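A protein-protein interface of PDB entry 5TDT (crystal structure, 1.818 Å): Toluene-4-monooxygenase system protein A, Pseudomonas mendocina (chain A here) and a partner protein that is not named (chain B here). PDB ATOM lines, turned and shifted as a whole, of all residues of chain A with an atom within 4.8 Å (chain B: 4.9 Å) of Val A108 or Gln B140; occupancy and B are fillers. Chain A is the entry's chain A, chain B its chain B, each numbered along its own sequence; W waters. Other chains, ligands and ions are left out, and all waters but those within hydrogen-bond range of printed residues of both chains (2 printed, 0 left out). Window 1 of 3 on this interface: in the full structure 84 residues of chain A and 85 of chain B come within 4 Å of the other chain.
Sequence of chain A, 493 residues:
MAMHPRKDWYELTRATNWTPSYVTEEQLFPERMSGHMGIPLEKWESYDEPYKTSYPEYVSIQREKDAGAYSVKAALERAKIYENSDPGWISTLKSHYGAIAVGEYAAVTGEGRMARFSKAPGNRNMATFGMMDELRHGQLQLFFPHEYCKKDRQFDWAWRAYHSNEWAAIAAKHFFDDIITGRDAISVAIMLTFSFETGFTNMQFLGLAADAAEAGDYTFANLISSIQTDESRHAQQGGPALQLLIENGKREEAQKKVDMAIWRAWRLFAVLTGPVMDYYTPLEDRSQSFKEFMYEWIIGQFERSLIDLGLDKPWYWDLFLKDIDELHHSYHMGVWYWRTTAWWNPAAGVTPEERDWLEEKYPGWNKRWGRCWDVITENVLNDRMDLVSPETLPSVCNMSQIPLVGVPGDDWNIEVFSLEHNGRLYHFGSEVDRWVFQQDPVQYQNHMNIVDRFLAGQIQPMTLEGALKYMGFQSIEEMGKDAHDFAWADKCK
OG1 of Thr A109 is in hydrogen-bond range of NE2 of Gln B140 (3.3 Å). The backbone carbonyl oxygen of Gly A112 sits at hydrogen-bond distance from the side-chain amide nitrogen of Gln B141, 2.9 Å away.
O of Ala B137 lies close to OE1 of Gln B140. The side-chain hydroxyl (OG) of Ser B149 sits at hydrogen-bond distance from a ring nitrogen (NE2) of His B33, at 2.9 Å. O of Gln B140 sits at hydrogen-bond distance from OG of Ser B149, at 2.7 Å. A ring nitrogen (NE2) of His B33 lies close to the backbone carbonyl oxygen (O) of Ala B143 (3.3 Å). The side-chain amide nitrogen of Gln B141 lies within hydrogen-bond range of the backbone carbonyl oxygen of Ala B137 (2.9 Å).
Among the printed residues, pairs that only touch across the chains: Gly A112 with Gln B140, Val A108 with Ile B153, Val A108 with Gln B140, Tyr A105 with His B33, Tyr A105 with Ser B149, Met A131 with Gln B140 and Leu A135 with Ile B153.
Glu A134 touches none of the printed residues of chain B. Of the printed residues of chain A, His B33 touches Tyr A105 (3.6 Å). Of chain A, only Val A108, Thr A109, Gly A112 and Met A131 come within 4 Å of Gln B140. Printed residues of chain A within 4 Å of Gln B141: Gly A112 (2.9 Å). The nearest printed residue of chain A that does not touch Gln B140 is Glu A111 (5.5 Å). The nearest printed residue of chain B that does not touch Tyr A105 is Ile B153 (4.6 Å).
Hydrophobic or aromatic side chains of chain B that line the printed part of chain A: His B33 and Ile B153. Printed residues of chain A that touch a printed residue of chain B: Tyr A105, Val A108, Thr A109, Gly A112, Met A131 and Leu A135. Among the printed residues, 9 pairs touch across the chains. Among the printed residues, no Asp or Glu carboxylate lies within 4 Å of a Lys or Arg side-chain nitrogen of the other chain.
Water W2 lies within hydrogen-bond range of OG1 of Thr A109 and O of Gln B141. Water W1 bridges the side-chain amide nitrogen of Gln B140 and the side-chain hydroxyl of Tyr A105.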
ATOM      1  N   GLU A 104      11.523  -1.362 -20.657  1.00  0.00           N
ATOM      2  CA  GLU A 104      10.825  -2.642 -20.610  1.00  0.00           C
ATOM      3  C   GLU A 104      11.233  -3.521 -21.780  1.00  0.00           C
ATOM      4  O   GLU A 104      11.459  -4.726 -21.623  1.00  0.00           O
ATOM      5  CB  GLU A 104       9.313  -2.419 -20.633  1.00  0.00           C
ATOM      6  CG  GLU A 104       8.809  -1.656 -19.442  1.00  0.00           C
ATOM      7  CD  GLU A 104       8.179  -2.549 -18.401  1.00  0.00           C
ATOM      8  OE1 GLU A 104       7.273  -2.063 -17.689  1.00  0.00           O
ATOM      9  OE2 GLU A 104       8.569  -3.740 -18.301  1.00  0.00           O
ATOM     10  N   TYR A 105      11.272  -2.946 -22.982  1.00  0.00           N
ATOM     11  CA  TYR A 105      11.691  -3.742 -24.129  1.00  0.00           C
ATOM     12  C   TYR A 105      13.116  -4.247 -23.938  1.00  0.00           C
ATOM     13  O   TYR A 105      13.429  -5.387 -24.302  1.00  0.00           O
ATOM     14  CB  TYR A 105      11.561  -2.940 -25.423  1.00  0.00           C
ATOM     15  CG  TYR A 105      11.829  -3.824 -26.596  1.00  0.00           C
ATOM     16  CD1 TYR A 105      10.890  -4.772 -26.990  1.00  0.00           C
ATOM     17  CD2 TYR A 105      13.043  -3.774 -27.271  1.00  0.00           C
ATOM     18  CE1 TYR A 105      11.132  -5.611 -28.046  1.00  0.00           C
ATOM     19  CE2 TYR A 105      13.293  -4.613 -28.338  1.00  0.00           C
ATOM     20  CZ  TYR A 105      12.338  -5.530 -28.718  1.00  0.00           C
ATOM     21  OH  TYR A 105      12.575  -6.393 -29.779  1.00  0.00           O
ATOM     22  N   ALA A 106      13.992  -3.426 -23.332  1.00  0.00           N
ATOM     23  CA  ALA A 106      15.352  -3.887 -23.046  1.00  0.00           C
ATOM     24  C   ALA A 106      15.351  -5.070 -22.077  1.00  0.00           C
ATOM     25  O   ALA A 106      16.217  -5.951 -22.167  1.00  0.00           O
ATOM     26  CB  ALA A 106      16.201  -2.733 -22.497  1.00  0.00           C
ATOM     27  N   ALA A 107      14.380  -5.129 -21.163  1.00  0.00           N
ATOM     28  CA  ALA A 107      14.311  -6.251 -20.233  1.00  0.00           C
ATOM     29  C   ALA A 107      14.088  -7.585 -20.939  1.00  0.00           C
ATOM     30  O   ALA A 107      14.431  -8.634 -20.378  1.00  0.00           O
ATOM     31  CB  ALA A 107      13.207  -6.013 -19.189  1.00  0.00           C
ATOM     32  N   VAL A 108      13.513  -7.582 -22.147  1.00  0.00           N
ATOM     33  CA  VAL A 108      13.449  -8.822 -22.921  1.00  0.00           C
ATOM     34  C   VAL A 108      14.839  -9.445 -23.037  1.00  0.00           C
ATOM     35  O   VAL A 108      15.009 -10.664 -22.901  1.00  0.00           O
ATOM     36  CB  VAL A 108      12.828  -8.568 -24.309  1.00  0.00           C
ATOM     37  CG1 VAL A 108      12.892  -9.837 -25.133  1.00  0.00           C
ATOM     38  CG2 VAL A 108      11.368  -8.076 -24.183  1.00  0.00           C
ATOM     39  N   THR A 109      15.859  -8.610 -23.255  1.00  0.00           N
ATOM     40  CA  THR A 109      17.219  -9.119 -23.425  1.00  0.00           C
ATOM     41  C   THR A 109      17.791  -9.680 -22.124  1.00  0.00           C
ATOM     42  O   THR A 109      18.518 -10.681 -22.151  1.00  0.00           O
ATOM     43  CB  THR A 109      18.115  -8.013 -23.993  1.00  0.00           C
ATOM     44  OG1 THR A 109      17.736  -7.767 -25.347  1.00  0.00           O
ATOM     45  CG2 THR A 109      19.604  -8.402 -23.941  1.00  0.00           C
ATOM     46  N   GLY A 110      17.502  -9.045 -20.980  1.00  0.00           N
ATOM     47  CA  GLY A 110      17.863  -9.648 -19.698  1.00  0.00           C
ATOM     48  C   GLY A 110      17.270 -11.039 -19.531  1.00  0.00           C
ATOM     49  O   GLY A 110      17.958 -11.983 -19.110  1.00  0.00           O
ATOM     50  N   GLU A 111      15.985 -11.184 -19.863  1.00  0.00           N
ATOM     51  CA  GLU A 111      15.343 -12.491 -19.798  1.00  0.00           C
ATOM     52  C   GLU A 111      15.923 -13.443 -20.849  1.00  0.00           C
ATOM     53  O   GLU A 111      16.137 -14.631 -20.576  1.00  0.00           O
ATOM     54  CB  GLU A 111      13.833 -12.335 -19.994  1.00  0.00           C
ATOM     55  CG  GLU A 111      13.098 -11.553 -18.860  1.00  0.00           C
ATOM     56  CD  GLU A 111      12.943 -12.338 -17.556  1.00  0.00           C
ATOM     57  OE1 GLU A 111      13.227 -13.558 -17.535  1.00  0.00           O
ATOM     58  OE2 GLU A 111      12.515 -11.731 -16.531  1.00  0.00           O
ATOM     59  N   GLY A 112      16.173 -12.947 -22.066  1.00  0.00           N
ATOM     60  CA  GLY A 112      16.793 -13.789 -23.084  1.00  0.00           C
ATOM     61  C   GLY A 112      18.168 -14.271 -22.672  1.00  0.00           C
ATOM     62  O   GLY A 112      18.560 -15.392 -22.998  1.00  0.00           O
ATOM     63  N   MET A 131      10.675 -13.292 -21.174  1.00  0.00           N
ATOM     64  CA  MET A 131      10.845 -12.598 -22.454  1.00  0.00           C
ATOM     65  C   MET A 131       9.505 -12.119 -22.998  1.00  0.00           C
ATOM     66  O   MET A 131       9.365 -10.972 -23.453  1.00  0.00           O
ATOM     67  CB  MET A 131      11.500 -13.523 -23.481  1.00  0.00           C
ATOM     68  CG  MET A 131      12.945 -13.889 -23.183  1.00  0.00           C
ATOM     69  SD  MET A 131      13.521 -15.264 -24.200  1.00  0.00           S
ATOM     70  CE  MET A 131      13.623 -14.506 -25.838  1.00  0.00           C
ATOM     71  N   GLU A 134       7.985  -9.132 -20.947  1.00  0.00           N
ATOM     72  CA  GLU A 134       8.538  -7.796 -21.156  1.00  0.00           C
ATOM     73  C   GLU A 134       8.226  -7.287 -22.554  1.00  0.00           C
ATOM     74  O   GLU A 134       8.115  -6.072 -22.757  1.00  0.00           O
ATOM     75  CB  GLU A 134      10.042  -7.781 -20.883  1.00  0.00           C
ATOM     76  CG  GLU A 134      10.443  -8.317 -19.495  1.00  0.00           C
ATOM     77  CD  GLU A 134       9.986  -7.445 -18.314  1.00  0.00           C
ATOM     78  OE1 GLU A 134       9.106  -6.557 -18.468  1.00  0.00           O
ATOM     79  OE2 GLU A 134      10.532  -7.653 -17.205  1.00  0.00           O
ATOM     80  N   LEU A 135       8.064  -8.191 -23.522  1.00  0.00           N
ATOM     81  CA  LEU A 135       7.534  -7.773 -24.819  1.00  0.00           C
ATOM     82  C   LEU A 135       6.161  -7.134 -24.647  1.00  0.00           C
ATOM     83  O   LEU A 135       5.884  -6.067 -25.207  1.00  0.00           O
ATOM     84  CB  LEU A 135       7.456  -8.966 -25.771  1.00  0.00           C
ATOM     85  CG  LEU A 135       6.961  -8.703 -27.195  1.00  0.00           C
ATOM     86  CD1 LEU A 135       7.911  -7.760 -27.921  1.00  0.00           C
ATOM     87  CD2 LEU A 135       6.836 -10.006 -27.979  1.00  0.00           C
ATOM     88  N   HIS B  33      15.770  -1.064 -30.506  1.00  0.00           N
ATOM     89  CA  HIS B  33      17.119  -1.367 -29.999  1.00  0.00           C
ATOM     90  C   HIS B  33      17.939  -0.079 -29.992  1.00  0.00           C
ATOM     91  O   HIS B  33      18.509   0.303 -31.016  1.00  0.00           O
ATOM     92  CB  HIS B  33      17.837  -2.389 -30.873  1.00  0.00           C
ATOM     93  CG  HIS B  33      17.394  -3.805 -30.686  1.00  0.00           C
ATOM     94  ND1 HIS B  33      16.784  -4.262 -29.536  1.00  0.00           N
ATOM     95  CD2 HIS B  33      17.511  -4.878 -31.502  1.00  0.00           C
ATOM     96  CE1 HIS B  33      16.528  -5.554 -29.656  1.00  0.00           C
ATOM     97  NE2 HIS B  33      16.954  -5.951 -30.842  1.00  0.00           N
ATOM     98  N   SER B 136      16.957 -19.896 -30.267  1.00  0.00           N
ATOM     99  CA  SER B 136      16.102 -18.773 -30.653  1.00  0.00           C
ATOM    100  C   SER B 136      16.288 -17.583 -29.717  1.00  0.00           C
ATOM    101  O   SER B 136      16.303 -16.429 -30.166  1.00  0.00           O
ATOM    102  CB  SER B 136      14.632 -19.201 -30.675  1.00  0.00           C
ATOM    103  OG  SER B 136      14.399 -20.211 -31.646  1.00  0.00           O
ATOM    104  N   ALA B 137      16.406 -17.838 -28.412  1.00  0.00           N
ATOM    105  CA  ALA B 137      16.621 -16.748 -27.468  1.00  0.00           C
ATOM    106  C   ALA B 137      17.956 -16.050 -27.717  1.00  0.00           C
ATOM    107  O   ALA B 137      18.072 -14.837 -27.496  1.00  0.00           O
ATOM    108  CB  ALA B 137      16.543 -17.261 -26.023  1.00  0.00           C
ATOM    109  N   TYR B 138      18.976 -16.790 -28.165  1.00  0.00           N
ATOM    110  CA  TYR B 138      20.247 -16.142 -28.493  1.00  0.00           C
ATOM    111  C   TYR B 138      20.088 -15.207 -29.689  1.00  0.00           C
ATOM    112  O   TYR B 138      20.563 -14.062 -29.669  1.00  0.00           O
ATOM    113  CB  TYR B 138      21.351 -17.171 -28.771  1.00  0.00           C
ATOM    114  CG  TYR B 138      22.669 -16.463 -28.970  1.00  0.00           C
ATOM    115  CD1 TYR B 138      23.323 -15.891 -27.884  1.00  0.00           C
ATOM    116  CD2 TYR B 138      23.229 -16.303 -30.242  1.00  0.00           C
ATOM    117  CE1 TYR B 138      24.518 -15.205 -28.037  1.00  0.00           C
ATOM    118  CE2 TYR B 138      24.442 -15.607 -30.410  1.00  0.00           C
ATOM    119  CZ  TYR B 138      25.076 -15.071 -29.303  1.00  0.00           C
ATOM    120  OH  TYR B 138      26.259 -14.375 -29.436  1.00  0.00           O
ATOM    121  N   VAL B 139      19.422 -15.670 -30.751  1.00  0.00           N
ATOM    122  CA  VAL B 139      19.232 -14.775 -31.888  1.00  0.00           C
ATOM    123  C   VAL B 139      18.417 -13.557 -31.455  1.00  0.00           C
ATOM    124  O   VAL B 139      18.687 -12.427 -31.884  1.00  0.00           O
ATOM    125  CB  VAL B 139      18.604 -15.511 -33.089  1.00  0.00           C
ATOM    126  CG1 VAL B 139      18.550 -14.581 -34.283  1.00  0.00           C
ATOM    127  CG2 VAL B 139      19.429 -16.736 -33.473  1.00  0.00           C
ATOM    128  N   GLN B 140      17.447 -13.758 -30.550  1.00  0.00           N
ATOM    129  CA  GLN B 140      16.678 -12.632 -30.022  1.00  0.00           C
ATOM    130  C   GLN B 140      17.598 -11.543 -29.486  1.00  0.00           C
ATOM    131  O   GLN B 140      17.506 -10.376 -29.894  1.00  0.00           O
ATOM    132  CB  GLN B 140      15.713 -13.102 -28.920  1.00  0.00           C
ATOM    133  CG  GLN B 140      15.045 -11.961 -28.122  1.00  0.00           C
ATOM    134  CD  GLN B 140      15.913 -11.398 -26.987  1.00  0.00           C
ATOM    135  OE1 GLN B 140      16.507 -12.150 -26.203  1.00  0.00           O
ATOM    136  NE2 GLN B 140      16.006 -10.059 -26.914  1.00  0.00           N
ATOM    137  N   GLN B 141      18.509 -11.915 -28.580  1.00  0.00           N
ATOM    138  CA  GLN B 141      19.284 -10.916 -27.846  1.00  0.00           C
ATOM    139  C   GLN B 141      20.388 -10.278 -28.682  1.00  0.00           C
ATOM    140  O   GLN B 141      20.847  -9.189 -28.316  1.00  0.00           O
ATOM    141  CB  GLN B 141      19.875 -11.522 -26.560  1.00  0.00           C
ATOM    142  CG  GLN B 141      20.866 -12.660 -26.770  1.00  0.00           C
ATOM    143  CD  GLN B 141      20.984 -13.541 -25.560  1.00  0.00           C
ATOM    144  OE1 GLN B 141      21.943 -13.448 -24.801  1.00  0.00           O
ATOM    145  NE2 GLN B 141      20.011 -14.409 -25.370  1.00  0.00           N
ATOM    146  N   MET B 142      20.819 -10.908 -29.788  1.00  0.00           N
ATOM    147  CA  MET B 142      21.889 -10.349 -30.623  1.00  0.00           C
ATOM    148  C   MET B 142      21.430  -9.610 -31.873  1.00  0.00           C
ATOM    149  O   MET B 142      22.237  -8.873 -32.452  1.00  0.00           O
ATOM    150  CB  MET B 142      22.883 -11.435 -31.070  1.00  0.00           C
ATOM    151  CG  MET B 142      23.429 -12.209 -29.904  1.00  0.00           C
ATOM    152  SD  MET B 142      24.231 -11.079 -28.704  1.00  0.00           S
ATOM    153  CE  MET B 142      25.237  -9.924 -29.688  1.00  0.00           C
ATOM    154  N   ALA B 143      20.188  -9.781 -32.298  1.00  0.00           N
ATOM    155  CA  ALA B 143      19.800  -9.321 -33.619  1.00  0.00           C
ATOM    156  C   ALA B 143      19.783  -7.796 -33.673  1.00  0.00           C
ATOM    157  O   ALA B 143      19.464  -7.134 -32.679  1.00  0.00           O
ATOM    158  CB  ALA B 143      18.428  -9.872 -33.996  1.00  0.00           C
ATOM    159  N   SER B 149      14.299  -9.238 -33.655  1.00  0.00           N
ATOM    160  CA  SER B 149      14.255  -9.862 -32.332  1.00  0.00           C
ATOM    161  C   SER B 149      12.847 -10.316 -31.937  1.00  0.00           C
ATOM    162  O   SER B 149      12.691 -11.362 -31.295  1.00  0.00           O
ATOM    163  CB  SER B 149      14.828  -8.913 -31.269  1.00  0.00           C
ATOM    164  OG  SER B 149      16.206  -8.625 -31.509  1.00  0.00           O
ATOM    165  N   CYS B 152      12.067 -13.584 -33.200  1.00  0.00           N
ATOM    166  CA  CYS B 152      12.783 -14.590 -32.424  1.00  0.00           C
ATOM    167  C   CYS B 152      12.126 -14.845 -31.073  1.00  0.00           C
ATOM    168  O   CYS B 152      12.167 -15.974 -30.581  1.00  0.00           O
ATOM    169  CB  CYS B 152      14.247 -14.173 -32.223  1.00  0.00           C
ATOM    170  SG  CYS B 152      15.213 -14.015 -33.753  1.00  0.00           S
ATOM    171  N   ILE B 153      11.554 -13.816 -30.440  1.00  0.00           N
ATOM    172  CA  ILE B 153      10.848 -14.029 -29.176  1.00  0.00           C
ATOM    173  C   ILE B 153       9.699 -15.011 -29.368  1.00  0.00           C
ATOM    174  O   ILE B 153       9.536 -15.970 -28.604  1.00  0.00           O
ATOM    175  CB  ILE B 153      10.325 -12.699 -28.602  1.00  0.00           C
ATOM    176  CG1 ILE B 153      11.454 -11.711 -28.300  1.00  0.00           C
ATOM    177  CG2 ILE B 153       9.486 -12.963 -27.327  1.00  0.00           C
ATOM    178  CD1 ILE B 153      10.909 -10.292 -28.032  1.00  0.00           C
HETATM  179  O   HOH W   1      14.579  -7.808 -28.029  1.00  0.00           O
HETATM  180  O   HOH W   2      19.669  -7.046 -26.941  1.00  0.00           O
